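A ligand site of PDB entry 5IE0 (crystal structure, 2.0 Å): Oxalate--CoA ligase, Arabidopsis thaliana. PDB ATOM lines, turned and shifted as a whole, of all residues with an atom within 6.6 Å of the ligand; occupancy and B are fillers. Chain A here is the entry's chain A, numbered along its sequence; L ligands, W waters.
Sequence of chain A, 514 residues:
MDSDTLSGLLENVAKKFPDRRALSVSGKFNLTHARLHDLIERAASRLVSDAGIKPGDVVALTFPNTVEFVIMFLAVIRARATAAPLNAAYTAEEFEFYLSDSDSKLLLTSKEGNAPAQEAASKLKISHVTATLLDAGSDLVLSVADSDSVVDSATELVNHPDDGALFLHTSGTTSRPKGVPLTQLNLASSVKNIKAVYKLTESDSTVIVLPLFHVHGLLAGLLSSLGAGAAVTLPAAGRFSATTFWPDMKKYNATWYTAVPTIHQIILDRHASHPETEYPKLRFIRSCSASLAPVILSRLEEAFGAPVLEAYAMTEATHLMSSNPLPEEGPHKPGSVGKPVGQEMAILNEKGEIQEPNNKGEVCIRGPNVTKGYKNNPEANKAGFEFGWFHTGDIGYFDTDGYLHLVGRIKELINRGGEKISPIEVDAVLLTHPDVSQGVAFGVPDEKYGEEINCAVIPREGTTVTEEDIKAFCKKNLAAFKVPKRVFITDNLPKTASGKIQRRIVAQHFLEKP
Water W4 lies within hydrogen-bond range of an oxygen (O2) of the ligand (2.6 Å), the side-chain hydroxyl of Ser 498 (2.6 Å) and the side-chain amino group of Lys 500 (3.2 Å). Water W2 lies within hydrogen-bond range of O4 of the ligand (2.6 Å), O of Ser 289 (2.7 Å) and O of Ala 313 (3.1 Å). Water W1 lies within hydrogen-bond range of N of Thr 315 (2.9 Å) and O1 of the ligand (2.9 Å). Water W3 lies within hydrogen-bond range of OG of Ser 289 (2.9 Å) and O2 of the ligand (3.4 Å).
OG of Ser 289 sits at hydrogen-bond distance from ND1 of His 216 (2.9 Å). N of His 319 lies within hydrogen-bond range of O of Met 314 (2.9 Å). The guanidinium group (NH2) of Arg 286 lies within hydrogen-bond range of a ring nitrogen (NE2) of His 319, at 3.0 Å. The guanidinium group (NH1) of Arg 286 sits at hydrogen-bond distance from a ring nitrogen (NE2) of His 216 (3.3 Å). N of Tyr 312 sits at hydrogen-bond distance from SG of Cys 288 (3.8 Å).
The side-chain hydroxyl (OG) of Ser 289 sits at hydrogen-bond distance from an oxygen (O6) of the ligand. A ring nitrogen (ND1) of His 319 sits at hydrogen-bond distance from an oxygen (O5) of the ligand, 2.7 Å away. An oxygen (O3) of the ligand is in hydrogen-bond range of the backbone NH (N) of His 216, 2.9 Å away. The backbone NH of Val 215 sits close to an oxygen (O3) of the ligand (3.3 Å). An oxygen (O1) of the ligand lies within salt-bridge range of the side-chain amino group of Lys 500 (3.2 Å). ND1 of His 214 sits close to O2 of the ligand, 3.3 Å away. N of Met 314 sits at hydrogen-bond distance from O5 of the ligand.
Merely in contact with the ligand: Cys 288, Ala 313, Thr 315 and Ser 498. Hydrophobic or aromatic side chains within 4 Å of the ligand: His 214, Val 215, His 216, Ala 313 and His 319. 11 residues have an atom within 4 Å of the ligand: His 214, Val 215, His 216, Cys 288, Ser 289, Ala 313, Met 314, Thr 315, His 319, Ser 498 and Lys 500. Along chain A the residues within 4 Å of the ligand span positions 214 to 500.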
ATOM      1  N   HIS A 169      21.710  35.656 -28.387  1.00  0.00           N
ATOM      2  CA  HIS A 169      20.390  36.101 -27.968  1.00  0.00           C
ATOM      3  C   HIS A 169      19.472  34.913 -27.696  1.00  0.00           C
ATOM      4  O   HIS A 169      19.635  33.847 -28.272  1.00  0.00           O
ATOM      5  CB  HIS A 169      19.748  37.007 -29.027  1.00  0.00           C
ATOM      6  CG  HIS A 169      20.280  38.400 -29.033  1.00  0.00           C
ATOM      7  ND1 HIS A 169      21.410  38.764 -29.717  1.00  0.00           N
ATOM      8  CD2 HIS A 169      19.821  39.531 -28.438  1.00  0.00           C
ATOM      9  CE1 HIS A 169      21.639  40.060 -29.554  1.00  0.00           C
ATOM     10  NE2 HIS A 169      20.686  40.547 -28.771  1.00  0.00           N
ATOM     11  N   PHE A 213      26.295  28.980 -35.065  1.00  0.00           N
ATOM     12  CA  PHE A 213      25.897  30.221 -34.393  1.00  0.00           C
ATOM     13  C   PHE A 213      24.930  29.965 -33.233  1.00  0.00           C
ATOM     14  O   PHE A 213      24.338  30.904 -32.684  1.00  0.00           O
ATOM     15  CB  PHE A 213      25.299  31.220 -35.404  1.00  0.00           C
ATOM     16  CG  PHE A 213      24.181  30.687 -36.242  1.00  0.00           C
ATOM     17  CD1 PHE A 213      22.870  30.699 -35.783  1.00  0.00           C
ATOM     18  CD2 PHE A 213      24.422  30.202 -37.523  1.00  0.00           C
ATOM     19  CE1 PHE A 213      21.840  30.220 -36.561  1.00  0.00           C
ATOM     20  CE2 PHE A 213      23.395  29.729 -38.314  1.00  0.00           C
ATOM     21  CZ  PHE A 213      22.098  29.736 -37.828  1.00  0.00           C
ATOM     22  N   HIS A 214      24.776  28.699 -32.861  1.00  0.00           N
ATOM     23  CA  HIS A 214      24.121  28.316 -31.607  1.00  0.00           C
ATOM     24  C   HIS A 214      25.097  27.479 -30.778  1.00  0.00           C
ATOM     25  O   HIS A 214      26.038  26.924 -31.329  1.00  0.00           O
ATOM     26  CB  HIS A 214      22.832  27.534 -31.876  1.00  0.00           C
ATOM     27  CG  HIS A 214      21.742  28.364 -32.494  1.00  0.00           C
ATOM     28  ND1 HIS A 214      21.236  29.489 -31.883  1.00  0.00           N
ATOM     29  CD2 HIS A 214      21.063  28.230 -33.662  1.00  0.00           C
ATOM     30  CE1 HIS A 214      20.292  30.015 -32.649  1.00  0.00           C
ATOM     31  NE2 HIS A 214      20.166  29.273 -33.730  1.00  0.00           N
ATOM     32  N   VAL A 215      24.900  27.414 -29.458  1.00  0.00           N
ATOM     33  CA  VAL A 215      25.913  26.809 -28.594  1.00  0.00           C
ATOM     34  C   VAL A 215      26.031  25.278 -28.701  1.00  0.00           C
ATOM     35  O   VAL A 215      27.057  24.733 -28.337  1.00  0.00           O
ATOM     36  CB  VAL A 215      25.699  27.178 -27.100  1.00  0.00           C
ATOM     37  CG1 VAL A 215      26.009  28.642 -26.869  1.00  0.00           C
ATOM     38  CG2 VAL A 215      24.290  26.859 -26.658  1.00  0.00           C
ATOM     39  N   HIS A 216      24.995  24.601 -29.184  1.00  0.00           N
ATOM     40  CA  HIS A 216      25.108  23.138 -29.319  1.00  0.00           C
ATOM     41  C   HIS A 216      26.237  22.774 -30.282  1.00  0.00           C
ATOM     42  O   HIS A 216      27.178  22.088 -29.911  1.00  0.00           O
ATOM     43  CB  HIS A 216      23.774  22.529 -29.773  1.00  0.00           C
ATOM     44  CG  HIS A 216      23.776  21.027 -29.814  1.00  0.00           C
ATOM     45  ND1 HIS A 216      22.621  20.286 -29.880  1.00  0.00           N
ATOM     46  CD2 HIS A 216      24.792  20.132 -29.804  1.00  0.00           C
ATOM     47  CE1 HIS A 216      22.914  19.002 -29.911  1.00  0.00           C
ATOM     48  NE2 HIS A 216      24.236  18.882 -29.869  1.00  0.00           N
ATOM     49  N   GLY A 217      26.143  23.237 -31.527  1.00  0.00           N
ATOM     50  CA  GLY A 217      27.175  22.968 -32.501  1.00  0.00           C
ATOM     51  C   GLY A 217      28.497  23.622 -32.143  1.00  0.00           C
ATOM     52  O   GLY A 217      29.559  23.033 -32.310  1.00  0.00           O
ATOM     53  N   VAL A 260      20.529  17.466 -32.834  1.00  0.00           N
ATOM     54  CA  VAL A 260      19.213  17.606 -32.229  1.00  0.00           C
ATOM     55  C   VAL A 260      18.319  16.486 -32.764  1.00  0.00           C
ATOM     56  O   VAL A 260      18.589  15.933 -33.817  1.00  0.00           O
ATOM     57  CB  VAL A 260      18.611  18.996 -32.534  1.00  0.00           C
ATOM     58  CG1 VAL A 260      19.511  20.092 -32.000  1.00  0.00           C
ATOM     59  CG2 VAL A 260      18.398  19.172 -34.025  1.00  0.00           C
ATOM     60  N   ARG A 286      25.324  11.492 -29.633  1.00  0.00           N
ATOM     61  CA  ARG A 286      24.770  12.404 -28.642  1.00  0.00           C
ATOM     62  C   ARG A 286      23.524  13.109 -29.162  1.00  0.00           C
ATOM     63  O   ARG A 286      23.440  13.463 -30.340  1.00  0.00           O
ATOM     64  CB  ARG A 286      25.816  13.444 -28.234  1.00  0.00           C
ATOM     65  CG  ARG A 286      25.372  14.443 -27.170  1.00  0.00           C
ATOM     66  CD  ARG A 286      26.522  15.395 -26.817  1.00  0.00           C
ATOM     67  NE  ARG A 286      26.195  16.309 -25.732  1.00  0.00           N
ATOM     68  CZ  ARG A 286      25.852  17.582 -25.890  1.00  0.00           C
ATOM     69  NH1 ARG A 286      25.772  18.104 -27.112  1.00  0.00           N
ATOM     70  NH2 ARG A 286      25.579  18.334 -24.830  1.00  0.00           N
ATOM     71  N   CYS A 288      20.744  16.400 -28.009  1.00  0.00           N
ATOM     72  CA  CYS A 288      20.553  17.524 -27.102  1.00  0.00           C
ATOM     73  C   CYS A 288      19.657  18.598 -27.727  1.00  0.00           C
ATOM     74  O   CYS A 288      19.311  18.500 -28.915  1.00  0.00           O
ATOM     75  CB  CYS A 288      21.908  18.118 -26.703  1.00  0.00           C
ATOM     76  SG  CYS A 288      21.885  19.210 -25.252  1.00  0.00           S
ATOM     77  N   SER A 289      19.306  19.604 -26.921  1.00  0.00           N
ATOM     78  CA  SER A 289      18.551  20.818 -27.304  1.00  0.00           C
ATOM     79  C   SER A 289      17.034  20.649 -27.278  1.00  0.00           C
ATOM     80  O   SER A 289      16.298  21.611 -27.068  1.00  0.00           O
ATOM     81  CB  SER A 289      18.967  21.328 -28.694  1.00  0.00           C
ATOM     82  OG  SER A 289      20.345  21.639 -28.747  1.00  0.00           O
ATOM     83  N   ALA A 290      16.549  19.427 -27.493  1.00  0.00           N
ATOM     84  CA  ALA A 290      15.126  19.127 -27.377  1.00  0.00           C
ATOM     85  C   ALA A 290      14.956  17.672 -26.966  1.00  0.00           C
ATOM     86  O   ALA A 290      15.810  16.841 -27.283  1.00  0.00           O
ATOM     87  CB  ALA A 290      14.387  19.417 -28.679  1.00  0.00           C
ATOM     88  N   TYR A 312      21.236  17.763 -21.803  1.00  0.00           N
ATOM     89  CA  TYR A 312      20.329  18.865 -21.526  1.00  0.00           C
ATOM     90  C   TYR A 312      21.146  20.140 -21.404  1.00  0.00           C
ATOM     91  O   TYR A 312      22.129  20.196 -20.652  1.00  0.00           O
ATOM     92  CB  TYR A 312      19.546  18.563 -20.251  1.00  0.00           C
ATOM     93  CG  TYR A 312      18.779  19.700 -19.625  1.00  0.00           C
ATOM     94  CD1 TYR A 312      17.844  20.424 -20.348  1.00  0.00           C
ATOM     95  CD2 TYR A 312      18.941  19.996 -18.275  1.00  0.00           C
ATOM     96  CE1 TYR A 312      17.121  21.451 -19.758  1.00  0.00           C
ATOM     97  CE2 TYR A 312      18.224  21.004 -17.677  1.00  0.00           C
ATOM     98  CZ  TYR A 312      17.323  21.725 -18.414  1.00  0.00           C
ATOM     99  OH  TYR A 312      16.631  22.736 -17.791  1.00  0.00           O
ATOM    100  N   ALA A 313      20.741  21.162 -22.161  1.00  0.00           N
ATOM    101  CA  ALA A 313      21.578  22.338 -22.366  1.00  0.00           C
ATOM    102  C   ALA A 313      20.781  23.574 -22.775  1.00  0.00           C
ATOM    103  O   ALA A 313      19.655  23.470 -23.261  1.00  0.00           O
ATOM    104  CB  ALA A 313      22.624  22.036 -23.423  1.00  0.00           C
ATOM    105  N   MET A 314      21.380  24.749 -22.587  1.00  0.00           N
ATOM    106  CA  MET A 314      20.787  26.000 -23.064  1.00  0.00           C
ATOM    107  C   MET A 314      21.852  27.092 -23.141  1.00  0.00           C
ATOM    108  O   MET A 314      22.918  26.967 -22.544  1.00  0.00           O
ATOM    109  CB  MET A 314      19.613  26.436 -22.170  1.00  0.00           C
ATOM    110  CG  MET A 314      20.007  26.903 -20.770  1.00  0.00           C
ATOM    111  SD  MET A 314      18.574  26.999 -19.657  1.00  0.00           S
ATOM    112  CE  MET A 314      17.581  28.265 -20.451  1.00  0.00           C
ATOM    113  N   THR A 315      21.540  28.158 -23.867  1.00  0.00           N
ATOM    114  CA  THR A 315      22.488  29.239 -24.113  1.00  0.00           C
ATOM    115  C   THR A 315      23.016  29.871 -22.830  1.00  0.00           C
ATOM    116  O   THR A 315      24.217  30.114 -22.702  1.00  0.00           O
ATOM    117  CB  THR A 315      21.840  30.345 -24.978  1.00  0.00           C
ATOM    118  OG1 THR A 315      21.323  29.770 -26.184  1.00  0.00           O
ATOM    119  CG2 THR A 315      22.863  31.416 -25.327  1.00  0.00           C
ATOM    120  N   THR A 318      25.930  28.237 -21.256  1.00  0.00           N
ATOM    121  CA  THR A 318      26.985  27.983 -22.233  1.00  0.00           C
ATOM    122  C   THR A 318      26.874  26.524 -22.691  1.00  0.00           C
ATOM    123  O   THR A 318      27.843  25.767 -22.657  1.00  0.00           O
ATOM    124  CB  THR A 318      28.390  28.279 -21.664  1.00  0.00           C
ATOM    125  OG1 THR A 318      28.364  29.536 -20.976  1.00  0.00           O
ATOM    126  CG2 THR A 318      29.433  28.348 -22.781  1.00  0.00           C
ATOM    127  N   HIS A 319      25.655  26.161 -23.081  1.00  0.00           N
ATOM    128  CA  HIS A 319      25.275  24.817 -23.513  1.00  0.00           C
ATOM    129  C   HIS A 319      25.109  23.864 -22.318  1.00  0.00           C
ATOM    130  O   HIS A 319      24.160  24.008 -21.552  1.00  0.00           O
ATOM    131  CB  HIS A 319      26.271  24.248 -24.528  1.00  0.00           C
ATOM    132  CG  HIS A 319      25.787  23.015 -25.240  1.00  0.00           C
ATOM    133  ND1 HIS A 319      24.542  22.937 -25.822  1.00  0.00           N
ATOM    134  CD2 HIS A 319      26.384  21.824 -25.450  1.00  0.00           C
ATOM    135  CE1 HIS A 319      24.386  21.742 -26.360  1.00  0.00           C
ATOM    136  NE2 HIS A 319      25.489  21.048 -26.153  1.00  0.00           N
ATOM    137  N   LEU A 320      26.022  22.910 -22.173  1.00  0.00           N
ATOM    138  CA  LEU A 320      25.798  21.734 -21.314  1.00  0.00           C
ATOM    139  C   LEU A 320      25.385  22.024 -19.868  1.00  0.00           C
ATOM    140  O   LEU A 320      26.064  22.758 -19.154  1.00  0.00           O
ATOM    141  CB  LEU A 320      27.053  20.849 -21.299  1.00  0.00           C
ATOM    142  CG  LEU A 320      26.973  19.584 -20.445  1.00  0.00           C
ATOM    143  CD1 LEU A 320      25.917  18.620 -20.983  1.00  0.00           C
ATOM    144  CD2 LEU A 320      28.334  18.886 -20.322  1.00  0.00           C
ATOM    145  N   SER A 498      18.106  25.945 -35.825  1.00  0.00           N
ATOM    146  CA  SER A 498      18.755  25.009 -34.906  1.00  0.00           C
ATOM    147  C   SER A 498      18.112  23.623 -34.954  1.00  0.00           C
ATOM    148  O   SER A 498      18.694  22.645 -34.478  1.00  0.00           O
ATOM    149  CB  SER A 498      18.707  25.557 -33.475  1.00  0.00           C
ATOM    150  OG  SER A 498      17.396  25.954 -33.123  1.00  0.00           O
ATOM    151  N   LYS A 500      14.563  23.042 -34.147  1.00  0.00           N
ATOM    152  CA  LYS A 500      13.495  22.891 -33.155  1.00  0.00           C
ATOM    153  C   LYS A 500      12.114  23.164 -33.725  1.00  0.00           C
ATOM    154  O   LYS A 500      11.944  24.066 -34.546  1.00  0.00           O
ATOM    155  CB  LYS A 500      13.747  23.817 -31.961  1.00  0.00           C
ATOM    156  CG  LYS A 500      15.113  23.678 -31.326  1.00  0.00           C
ATOM    157  CD  LYS A 500      15.276  24.677 -30.198  1.00  0.00           C
ATOM    158  CE  LYS A 500      16.696  24.714 -29.677  1.00  0.00           C
ATOM    159  NZ  LYS A 500      16.865  25.759 -28.632  1.00  0.00           N
HETATM  160  O1  LIG L   1      19.594  27.347 -28.140  1.00  0.00           O
HETATM  161  O2  LIG L   1      20.058  26.887 -30.219  1.00  0.00           O
HETATM  162  C1  LIG L   1      20.155  26.621 -28.997  1.00  0.00           C
HETATM  163  C2  LIG L   1      20.922  25.393 -28.585  1.00  0.00           C
HETATM  164  O3  LIG L   1      22.303  25.591 -28.679  1.00  0.00           O
HETATM  165  C3  LIG L   1      20.491  24.968 -27.209  1.00  0.00           C
HETATM  166  O4  LIG L   1      19.309  24.238 -27.415  1.00  0.00           O
HETATM  167  C4  LIG L   1      21.525  24.058 -26.581  1.00  0.00           C
HETATM  168  O5  LIG L   1      22.406  24.540 -25.830  1.00  0.00           O
HETATM  169  O6  LIG L   1      21.505  22.825 -26.796  1.00  0.00           O
HETATM  170  O   HOH W   1      19.104  27.743 -25.334  1.00  0.00           O
HETATM  171  O   HOH W   2      17.597  23.477 -25.622  1.00  0.00           O
HETATM  172  O   HOH W   3      20.260  23.560 -30.900  1.00  0.00           O
HETATM  173  O   HOH W   4      17.787  27.602 -31.142  1.00  0.00           O
